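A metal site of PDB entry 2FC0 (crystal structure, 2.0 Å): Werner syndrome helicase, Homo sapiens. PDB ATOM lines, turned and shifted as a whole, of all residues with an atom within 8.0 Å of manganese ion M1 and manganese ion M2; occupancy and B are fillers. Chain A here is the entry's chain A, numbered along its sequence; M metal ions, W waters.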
ATOM      1  N   PHE A  50      34.833 -16.785  -1.084  1.00  0.00           N
ATOM      2  CA  PHE A  50      34.555 -17.594  -2.265  1.00  0.00           C
ATOM      3  C   PHE A  50      33.290 -18.433  -2.161  1.00  0.00           C
ATOM      4  O   PHE A  50      32.950 -18.937  -1.087  1.00  0.00           O
ATOM      5  CB  PHE A  50      35.758 -18.519  -2.499  1.00  0.00           C
ATOM      6  CG  PHE A  50      35.557 -19.529  -3.601  1.00  0.00           C
ATOM      7  CD1 PHE A  50      36.075 -19.301  -4.874  1.00  0.00           C
ATOM      8  CD2 PHE A  50      34.874 -20.715  -3.357  1.00  0.00           C
ATOM      9  CE1 PHE A  50      35.899 -20.228  -5.890  1.00  0.00           C
ATOM     10  CE2 PHE A  50      34.685 -21.651  -4.368  1.00  0.00           C
ATOM     11  CZ  PHE A  50      35.203 -21.414  -5.643  1.00  0.00           C
ATOM     12  N   ASP A  51      32.582 -18.574  -3.289  1.00  0.00           N
ATOM     13  CA  ASP A  51      31.387 -19.397  -3.378  1.00  0.00           C
ATOM     14  C   ASP A  51      31.110 -19.582  -4.869  1.00  0.00           C
ATOM     15  O   ASP A  51      31.687 -18.890  -5.696  1.00  0.00           O
ATOM     16  CB  ASP A  51      30.161 -18.736  -2.707  1.00  0.00           C
ATOM     17  CG  ASP A  51      29.036 -19.735  -2.458  1.00  0.00           C
ATOM     18  OD1 ASP A  51      27.875 -19.319  -2.262  1.00  0.00           O
ATOM     19  OD2 ASP A  51      29.339 -20.951  -2.444  1.00  0.00           O
ATOM     20  N   MET A  52      30.289 -20.543  -5.182  1.00  0.00           N
ATOM     21  CA  MET A  52      29.960 -20.745  -6.573  1.00  0.00           C
ATOM     22  C   MET A  52      28.574 -21.289  -6.587  1.00  0.00           C
ATOM     23  O   MET A  52      28.117 -21.854  -5.582  1.00  0.00           O
ATOM     24  CB  MET A  52      30.949 -21.692  -7.247  1.00  0.00           C
ATOM     25  CG  MET A  52      31.241 -22.973  -6.516  1.00  0.00           C
ATOM     26  SD  MET A  52      32.581 -23.858  -7.359  1.00  0.00           S
ATOM     27  CE  MET A  52      31.861 -25.475  -7.461  1.00  0.00           C
ATOM     28  N   GLU A  53      27.926 -21.082  -7.690  1.00  0.00           N
ATOM     29  CA  GLU A  53      26.557 -21.525  -7.857  1.00  0.00           C
ATOM     30  C   GLU A  53      26.390 -22.306  -9.141  1.00  0.00           C
ATOM     31  O   GLU A  53      27.187 -22.181 -10.072  1.00  0.00           O
ATOM     32  CB  GLU A  53      25.625 -20.322  -7.910  1.00  0.00           C
ATOM     33  CG  GLU A  53      25.767 -19.291  -6.787  1.00  0.00           C
ATOM     34  CD  GLU A  53      25.322 -19.810  -5.436  1.00  0.00           C
ATOM     35  OE1 GLU A  53      24.419 -20.674  -5.403  1.00  0.00           O
ATOM     36  OE2 GLU A  53      25.854 -19.332  -4.416  1.00  0.00           O
ATOM     37  N   TRP A  54      25.342 -23.115  -9.208  1.00  0.00           N
ATOM     38  CA  TRP A  54      25.032 -23.896 -10.399  1.00  0.00           C
ATOM     39  C   TRP A  54      23.530 -24.134 -10.459  1.00  0.00           C
ATOM     40  O   TRP A  54      22.849 -24.156  -9.442  1.00  0.00           O
ATOM     41  CB  TRP A  54      25.786 -25.231 -10.417  1.00  0.00           C
ATOM     42  CG  TRP A  54      25.568 -26.068  -9.198  1.00  0.00           C
ATOM     43  CD1 TRP A  54      24.516 -26.907  -8.963  1.00  0.00           C
ATOM     44  CD2 TRP A  54      26.398 -26.103  -8.037  1.00  0.00           C
ATOM     45  NE1 TRP A  54      24.640 -27.461  -7.704  1.00  0.00           N
ATOM     46  CE2 TRP A  54      25.777 -26.985  -7.118  1.00  0.00           C
ATOM     47  CE3 TRP A  54      27.594 -25.473  -7.668  1.00  0.00           C
ATOM     48  CZ2 TRP A  54      26.329 -27.251  -5.853  1.00  0.00           C
ATOM     49  CZ3 TRP A  54      28.135 -25.732  -6.422  1.00  0.00           C
ATOM     50  CH2 TRP A  54      27.505 -26.618  -5.530  1.00  0.00           C
ATOM     51  N   LEU A  68      28.425 -19.894 -12.003  1.00  0.00           N
ATOM     52  CA  LEU A  68      28.863 -18.631 -11.436  1.00  0.00           C
ATOM     53  C   LEU A  68      29.901 -18.813 -10.337  1.00  0.00           C
ATOM     54  O   LEU A  68      29.817 -19.745  -9.537  1.00  0.00           O
ATOM     55  CB  LEU A  68      27.641 -17.893 -10.865  1.00  0.00           C
ATOM     56  CG  LEU A  68      27.827 -16.520 -10.211  1.00  0.00           C
ATOM     57  CD1 LEU A  68      28.201 -15.478 -11.266  1.00  0.00           C
ATOM     58  CD2 LEU A  68      26.516 -16.118  -9.509  1.00  0.00           C
ATOM     59  N   GLN A  70      31.892 -16.510  -7.363  1.00  0.00           N
ATOM     60  CA  GLN A  70      31.899 -15.243  -6.658  1.00  0.00           C
ATOM     61  C   GLN A  70      33.127 -15.088  -5.772  1.00  0.00           C
ATOM     62  O   GLN A  70      33.490 -16.014  -5.035  1.00  0.00           O
ATOM     63  CB  GLN A  70      30.648 -15.108  -5.772  1.00  0.00           C
ATOM     64  CG  GLN A  70      29.324 -15.380  -6.466  1.00  0.00           C
ATOM     65  CD  GLN A  70      28.805 -16.792  -6.194  1.00  0.00           C
ATOM     66  OE1 GLN A  70      28.998 -17.697  -7.007  1.00  0.00           O
ATOM     67  NE2 GLN A  70      28.158 -16.978  -5.045  1.00  0.00           N
ATOM     68  N   GLY A 106      35.473 -20.236   2.589  1.00  0.00           N
ATOM     69  CA  GLY A 106      34.072 -20.551   2.399  1.00  0.00           C
ATOM     70  C   GLY A 106      33.658 -21.780   3.202  1.00  0.00           C
ATOM     71  O   GLY A 106      34.473 -22.372   3.895  1.00  0.00           O
ATOM     72  N   VAL A 107      32.379 -22.141   3.110  1.00  0.00           N
ATOM     73  CA  VAL A 107      31.861 -23.315   3.801  1.00  0.00           C
ATOM     74  C   VAL A 107      31.421 -24.312   2.738  1.00  0.00           C
ATOM     75  O   VAL A 107      30.632 -23.987   1.851  1.00  0.00           O
ATOM     76  CB  VAL A 107      30.650 -22.955   4.703  1.00  0.00           C
ATOM     77  CG1 VAL A 107      29.980 -24.227   5.207  1.00  0.00           C
ATOM     78  CG2 VAL A 107      31.111 -22.114   5.879  1.00  0.00           C
ATOM     79  N   GLY A 108      31.935 -25.542   2.849  1.00  0.00           N
ATOM     80  CA  GLY A 108      31.607 -26.566   1.875  1.00  0.00           C
ATOM     81  C   GLY A 108      32.503 -26.365   0.667  1.00  0.00           C
ATOM     82  O   GLY A 108      32.194 -26.803  -0.452  1.00  0.00           O
ATOM     83  N   ILE A 109      33.624 -25.695   0.896  1.00  0.00           N
ATOM     84  CA  ILE A 109      34.583 -25.381  -0.153  1.00  0.00           C
ATOM     85  C   ILE A 109      35.365 -26.577  -0.703  1.00  0.00           C
ATOM     86  O   ILE A 109      35.836 -26.533  -1.840  1.00  0.00           O
ATOM     87  CB  ILE A 109      35.543 -24.256   0.320  1.00  0.00           C
ATOM     88  CG1 ILE A 109      36.221 -23.605  -0.895  1.00  0.00           C
ATOM     89  CG2 ILE A 109      36.564 -24.808   1.296  1.00  0.00           C
ATOM     90  CD1 ILE A 109      36.914 -22.292  -0.572  1.00  0.00           C
ATOM     91  N   ASP A 112      33.297 -27.791  -3.375  1.00  0.00           N
ATOM     92  CA  ASP A 112      33.379 -26.918  -4.537  1.00  0.00           C
ATOM     93  C   ASP A 112      34.652 -27.298  -5.298  1.00  0.00           C
ATOM     94  O   ASP A 112      34.654 -27.343  -6.525  1.00  0.00           O
ATOM     95  CB  ASP A 112      33.475 -25.439  -4.131  1.00  0.00           C
ATOM     96  CG  ASP A 112      32.195 -24.922  -3.484  1.00  0.00           C
ATOM     97  OD1 ASP A 112      31.097 -25.281  -3.948  1.00  0.00           O
ATOM     98  OD2 ASP A 112      32.308 -24.144  -2.518  1.00  0.00           O
ATOM     99  N   LEU A 146      27.128 -22.176   6.519  1.00  0.00           N
ATOM    100  CA  LEU A 146      27.415 -20.755   6.336  1.00  0.00           C
ATOM    101  C   LEU A 146      26.401 -19.932   7.138  1.00  0.00           C
ATOM    102  O   LEU A 146      26.760 -18.951   7.790  1.00  0.00           O
ATOM    103  CB  LEU A 146      27.353 -20.392   4.848  1.00  0.00           C
ATOM    104  CG  LEU A 146      27.831 -18.982   4.484  1.00  0.00           C
ATOM    105  CD1 LEU A 146      29.293 -18.807   4.898  1.00  0.00           C
ATOM    106  CD2 LEU A 146      27.665 -18.773   2.981  1.00  0.00           C
ATOM    107  N   LEU A 158      20.959 -15.675   6.488  1.00  0.00           N
ATOM    108  CA  LEU A 158      21.109 -15.536   5.044  1.00  0.00           C
ATOM    109  C   LEU A 158      19.749 -15.495   4.347  1.00  0.00           C
ATOM    110  O   LEU A 158      18.797 -16.130   4.808  1.00  0.00           O
ATOM    111  CB  LEU A 158      21.909 -16.713   4.478  1.00  0.00           C
ATOM    112  CG  LEU A 158      23.357 -16.873   4.951  1.00  0.00           C
ATOM    113  CD1 LEU A 158      23.930 -18.162   4.399  1.00  0.00           C
ATOM    114  CD2 LEU A 158      24.165 -15.676   4.477  1.00  0.00           C
ATOM    115  N   ARG A 165      17.826 -19.074  -4.476  1.00  0.00           N
ATOM    116  CA  ARG A 165      18.994 -19.893  -4.225  1.00  0.00           C
ATOM    117  C   ARG A 165      19.065 -21.104  -5.125  1.00  0.00           C
ATOM    118  O   ARG A 165      20.152 -21.589  -5.446  1.00  0.00           O
ATOM    119  CB  ARG A 165      19.049 -20.330  -2.755  1.00  0.00           C
ATOM    120  CG  ARG A 165      19.552 -19.251  -1.839  1.00  0.00           C
ATOM    121  CD  ARG A 165      19.968 -19.790  -0.489  1.00  0.00           C
ATOM    122  NE  ARG A 165      20.442 -18.718   0.376  1.00  0.00           N
ATOM    123  CZ  ARG A 165      21.532 -17.992   0.131  1.00  0.00           C
ATOM    124  NH1 ARG A 165      21.879 -17.036   0.975  1.00  0.00           N
ATOM    125  NH2 ARG A 165      22.273 -18.238  -0.933  1.00  0.00           N
ATOM    126  N   TRP A 169      20.917 -20.509 -12.374  1.00  0.00           N
ATOM    127  CA  TRP A 169      22.121 -19.688 -12.383  1.00  0.00           C
ATOM    128  C   TRP A 169      22.862 -19.597 -13.710  1.00  0.00           C
ATOM    129  O   TRP A 169      23.749 -18.767 -13.851  1.00  0.00           O
ATOM    130  CB  TRP A 169      23.083 -20.174 -11.287  1.00  0.00           C
ATOM    131  CG  TRP A 169      22.526 -19.984  -9.905  1.00  0.00           C
ATOM    132  CD1 TRP A 169      21.907 -20.925  -9.127  1.00  0.00           C
ATOM    133  CD2 TRP A 169      22.519 -18.771  -9.143  1.00  0.00           C
ATOM    134  NE1 TRP A 169      21.521 -20.374  -7.926  1.00  0.00           N
ATOM    135  CE2 TRP A 169      21.878 -19.045  -7.910  1.00  0.00           C
ATOM    136  CE3 TRP A 169      22.993 -17.465  -9.380  1.00  0.00           C
ATOM    137  CZ2 TRP A 169      21.708 -18.076  -6.918  1.00  0.00           C
ATOM    138  CZ3 TRP A 169      22.815 -16.496  -8.394  1.00  0.00           C
ATOM    139  CH2 TRP A 169      22.176 -16.803  -7.178  1.00  0.00           C
ATOM    140  N   TYR A 181      21.993 -12.296  -3.756  1.00  0.00           N
ATOM    141  CA  TYR A 181      22.172 -13.585  -3.086  1.00  0.00           C
ATOM    142  C   TYR A 181      23.585 -14.117  -3.265  1.00  0.00           C
ATOM    143  O   TYR A 181      24.250 -14.502  -2.291  1.00  0.00           O
ATOM    144  CB  TYR A 181      21.178 -14.620  -3.636  1.00  0.00           C
ATOM    145  CG  TYR A 181      19.848 -14.682  -2.930  1.00  0.00           C
ATOM    146  CD1 TYR A 181      19.035 -13.546  -2.816  1.00  0.00           C
ATOM    147  CD2 TYR A 181      19.369 -15.889  -2.409  1.00  0.00           C
ATOM    148  CE1 TYR A 181      17.780 -13.617  -2.183  1.00  0.00           C
ATOM    149  CE2 TYR A 181      18.132 -15.971  -1.787  1.00  0.00           C
ATOM    150  CZ  TYR A 181      17.342 -14.835  -1.672  1.00  0.00           C
ATOM    151  OH  TYR A 181      16.118 -14.917  -1.054  1.00  0.00           O
ATOM    152  N   ALA A 182      24.035 -14.160  -4.518  1.00  0.00           N
ATOM    153  CA  ALA A 182      25.365 -14.672  -4.839  1.00  0.00           C
ATOM    154  C   ALA A 182      26.512 -13.861  -4.244  1.00  0.00           C
ATOM    155  O   ALA A 182      27.454 -14.433  -3.702  1.00  0.00           O
ATOM    156  CB  ALA A 182      25.527 -14.777  -6.372  1.00  0.00           C
ATOM    157  N   ALA A 183      26.444 -12.534  -4.349  1.00  0.00           N
ATOM    158  CA  ALA A 183      27.504 -11.691  -3.808  1.00  0.00           C
ATOM    159  C   ALA A 183      27.552 -11.818  -2.289  1.00  0.00           C
ATOM    160  O   ALA A 183      28.633 -11.816  -1.696  1.00  0.00           O
ATOM    161  CB  ALA A 183      27.275 -10.234  -4.204  1.00  0.00           C
ATOM    162  N   THR A 184      26.396 -11.919  -1.666  1.00  0.00           N
ATOM    163  CA  THR A 184      26.365 -12.036  -0.215  1.00  0.00           C
ATOM    164  C   THR A 184      26.979 -13.328   0.329  1.00  0.00           C
ATOM    165  O   THR A 184      27.548 -13.315   1.418  1.00  0.00           O
ATOM    166  CB  THR A 184      24.917 -11.841   0.311  1.00  0.00           C
ATOM    167  OG1 THR A 184      24.396 -10.603  -0.186  1.00  0.00           O
ATOM    168  CG2 THR A 184      24.907 -11.785   1.843  1.00  0.00           C
ATOM    169  N   ASP A 185      26.918 -14.450  -0.426  1.00  0.00           N
ATOM    170  CA  ASP A 185      27.516 -15.702   0.035  1.00  0.00           C
ATOM    171  C   ASP A 185      29.037 -15.562   0.118  1.00  0.00           C
ATOM    172  O   ASP A 185      29.674 -16.063   1.058  1.00  0.00           O
ATOM    173  CB  ASP A 185      27.164 -16.884  -0.909  1.00  0.00           C
ATOM    174  CG  ASP A 185      25.724 -17.325  -0.758  1.00  0.00           C
ATOM    175  OD1 ASP A 185      25.094 -17.020   0.280  1.00  0.00           O
ATOM    176  OD2 ASP A 185      25.214 -17.991  -1.684  1.00  0.00           O
ATOM    177  N   ALA A 186      29.610 -14.858  -0.851  1.00  0.00           N
ATOM    178  CA  ALA A 186      31.054 -14.644  -0.890  1.00  0.00           C
ATOM    179  C   ALA A 186      31.462 -13.646   0.190  1.00  0.00           C
ATOM    180  O   ALA A 186      32.463 -13.833   0.878  1.00  0.00           O
ATOM    181  CB  ALA A 186      31.477 -14.119  -2.266  1.00  0.00           C
HETATM  182 MN    MN M   1      25.940 -19.805  -2.474  1.00  0.00          MN
HETATM  183 MN    MN M   2      28.185 -22.706  -1.814  1.00  0.00          MN
HETATM  184  O   HOH W   1      30.052 -23.847  -1.015  1.00  0.00           O
HETATM  185  O   HOH W   2      28.734 -23.890  -3.903  1.00  0.00           O
HETATM  186  O   HOH W   3      26.091 -20.350  -0.325  1.00  0.00           O
HETATM  187  O   HOH W   4      28.200 -21.941   0.332  1.00  0.00           O
HETATM  188  O   HOH W   5      23.791 -20.563  -2.586  1.00  0.00           O
HETATM  189  O   HOH W   6      25.345 -23.720  -1.669  1.00  0.00           O
HETATM  190  O   HOH W   7      26.584 -21.790  -3.254  1.00  0.00           O
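Manganese ion M2 is bound by OD2 of Asp 51 (2.2 Å), water W4 (2.3 Å), water W1 (2.3 Å), water W7 (2.3 Å) and water W2 (2.5 Å).
Manganese ion M1 is bound by OE2 of Glu 53. Manganese ion M1 is bound by the side-chain carboxylate (OD1) of Asp 51. OD2 of Asp 185 binds manganese ion M1, at 2.1 Å. Manganese ion M1 is bound by water W3 (2.2 Å). Water W7 is bound to manganese ion M1. Manganese ion M1 is bound by water W5, 2.3 Å away. Manganese ion M1 has six donor atoms within binding distance.
Within 4 Å of manganese ion M1: Asp 51, Glu 53 and Asp 185. The nearest printed residue that does not touch manganese ion M1 is Arg 165 (4.3 Å).
The backbone carbonyl oxygen (O) of Asp 51 lies within hydrogen-bond range of the backbone NH (N) of Gln 70 (2.9 Å). The backbone NH of Glu 53 lies within hydrogen-bond range of the backbone carbonyl oxygen of Leu 68, at 3.0 Å. OE2 of Glu 53 lies close to NE2 of Gln 70, 3.4 Å away. OD1 of Asp 185 is in salt-bridge range of NH1 of Arg 165 (3.3 Å).
Merely in contact with manganese ion M2: Met 52. Within 4 Å of manganese ion M2: Asp 51 and Met 52. The nearest printed residue that does not touch manganese ion M2 is Asp 112 (4.4 Å).
Water W5 lies within hydrogen-bond range of the side-chain carboxylate (OE1) of Glu 53 (2.9 Å) and the guanidinium group (NH2) of Arg 165 (3.2 Å). Water W7 bridges the backbone carbonyl oxygen of Met 52 and the side-chain carboxylate of Glu 53. Water W2 lies within hydrogen-bond range of the backbone carbonyl oxygen (O) of Met 52 (2.7 Å) and the side-chain carboxylate (OD1) of Asp 112 (2.7 Å). Water W1 bridges the side-chain carboxylate of Asp 112 (2.7 Å) and the backbone carbonyl oxygen of Val 107 (2.9 Å).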
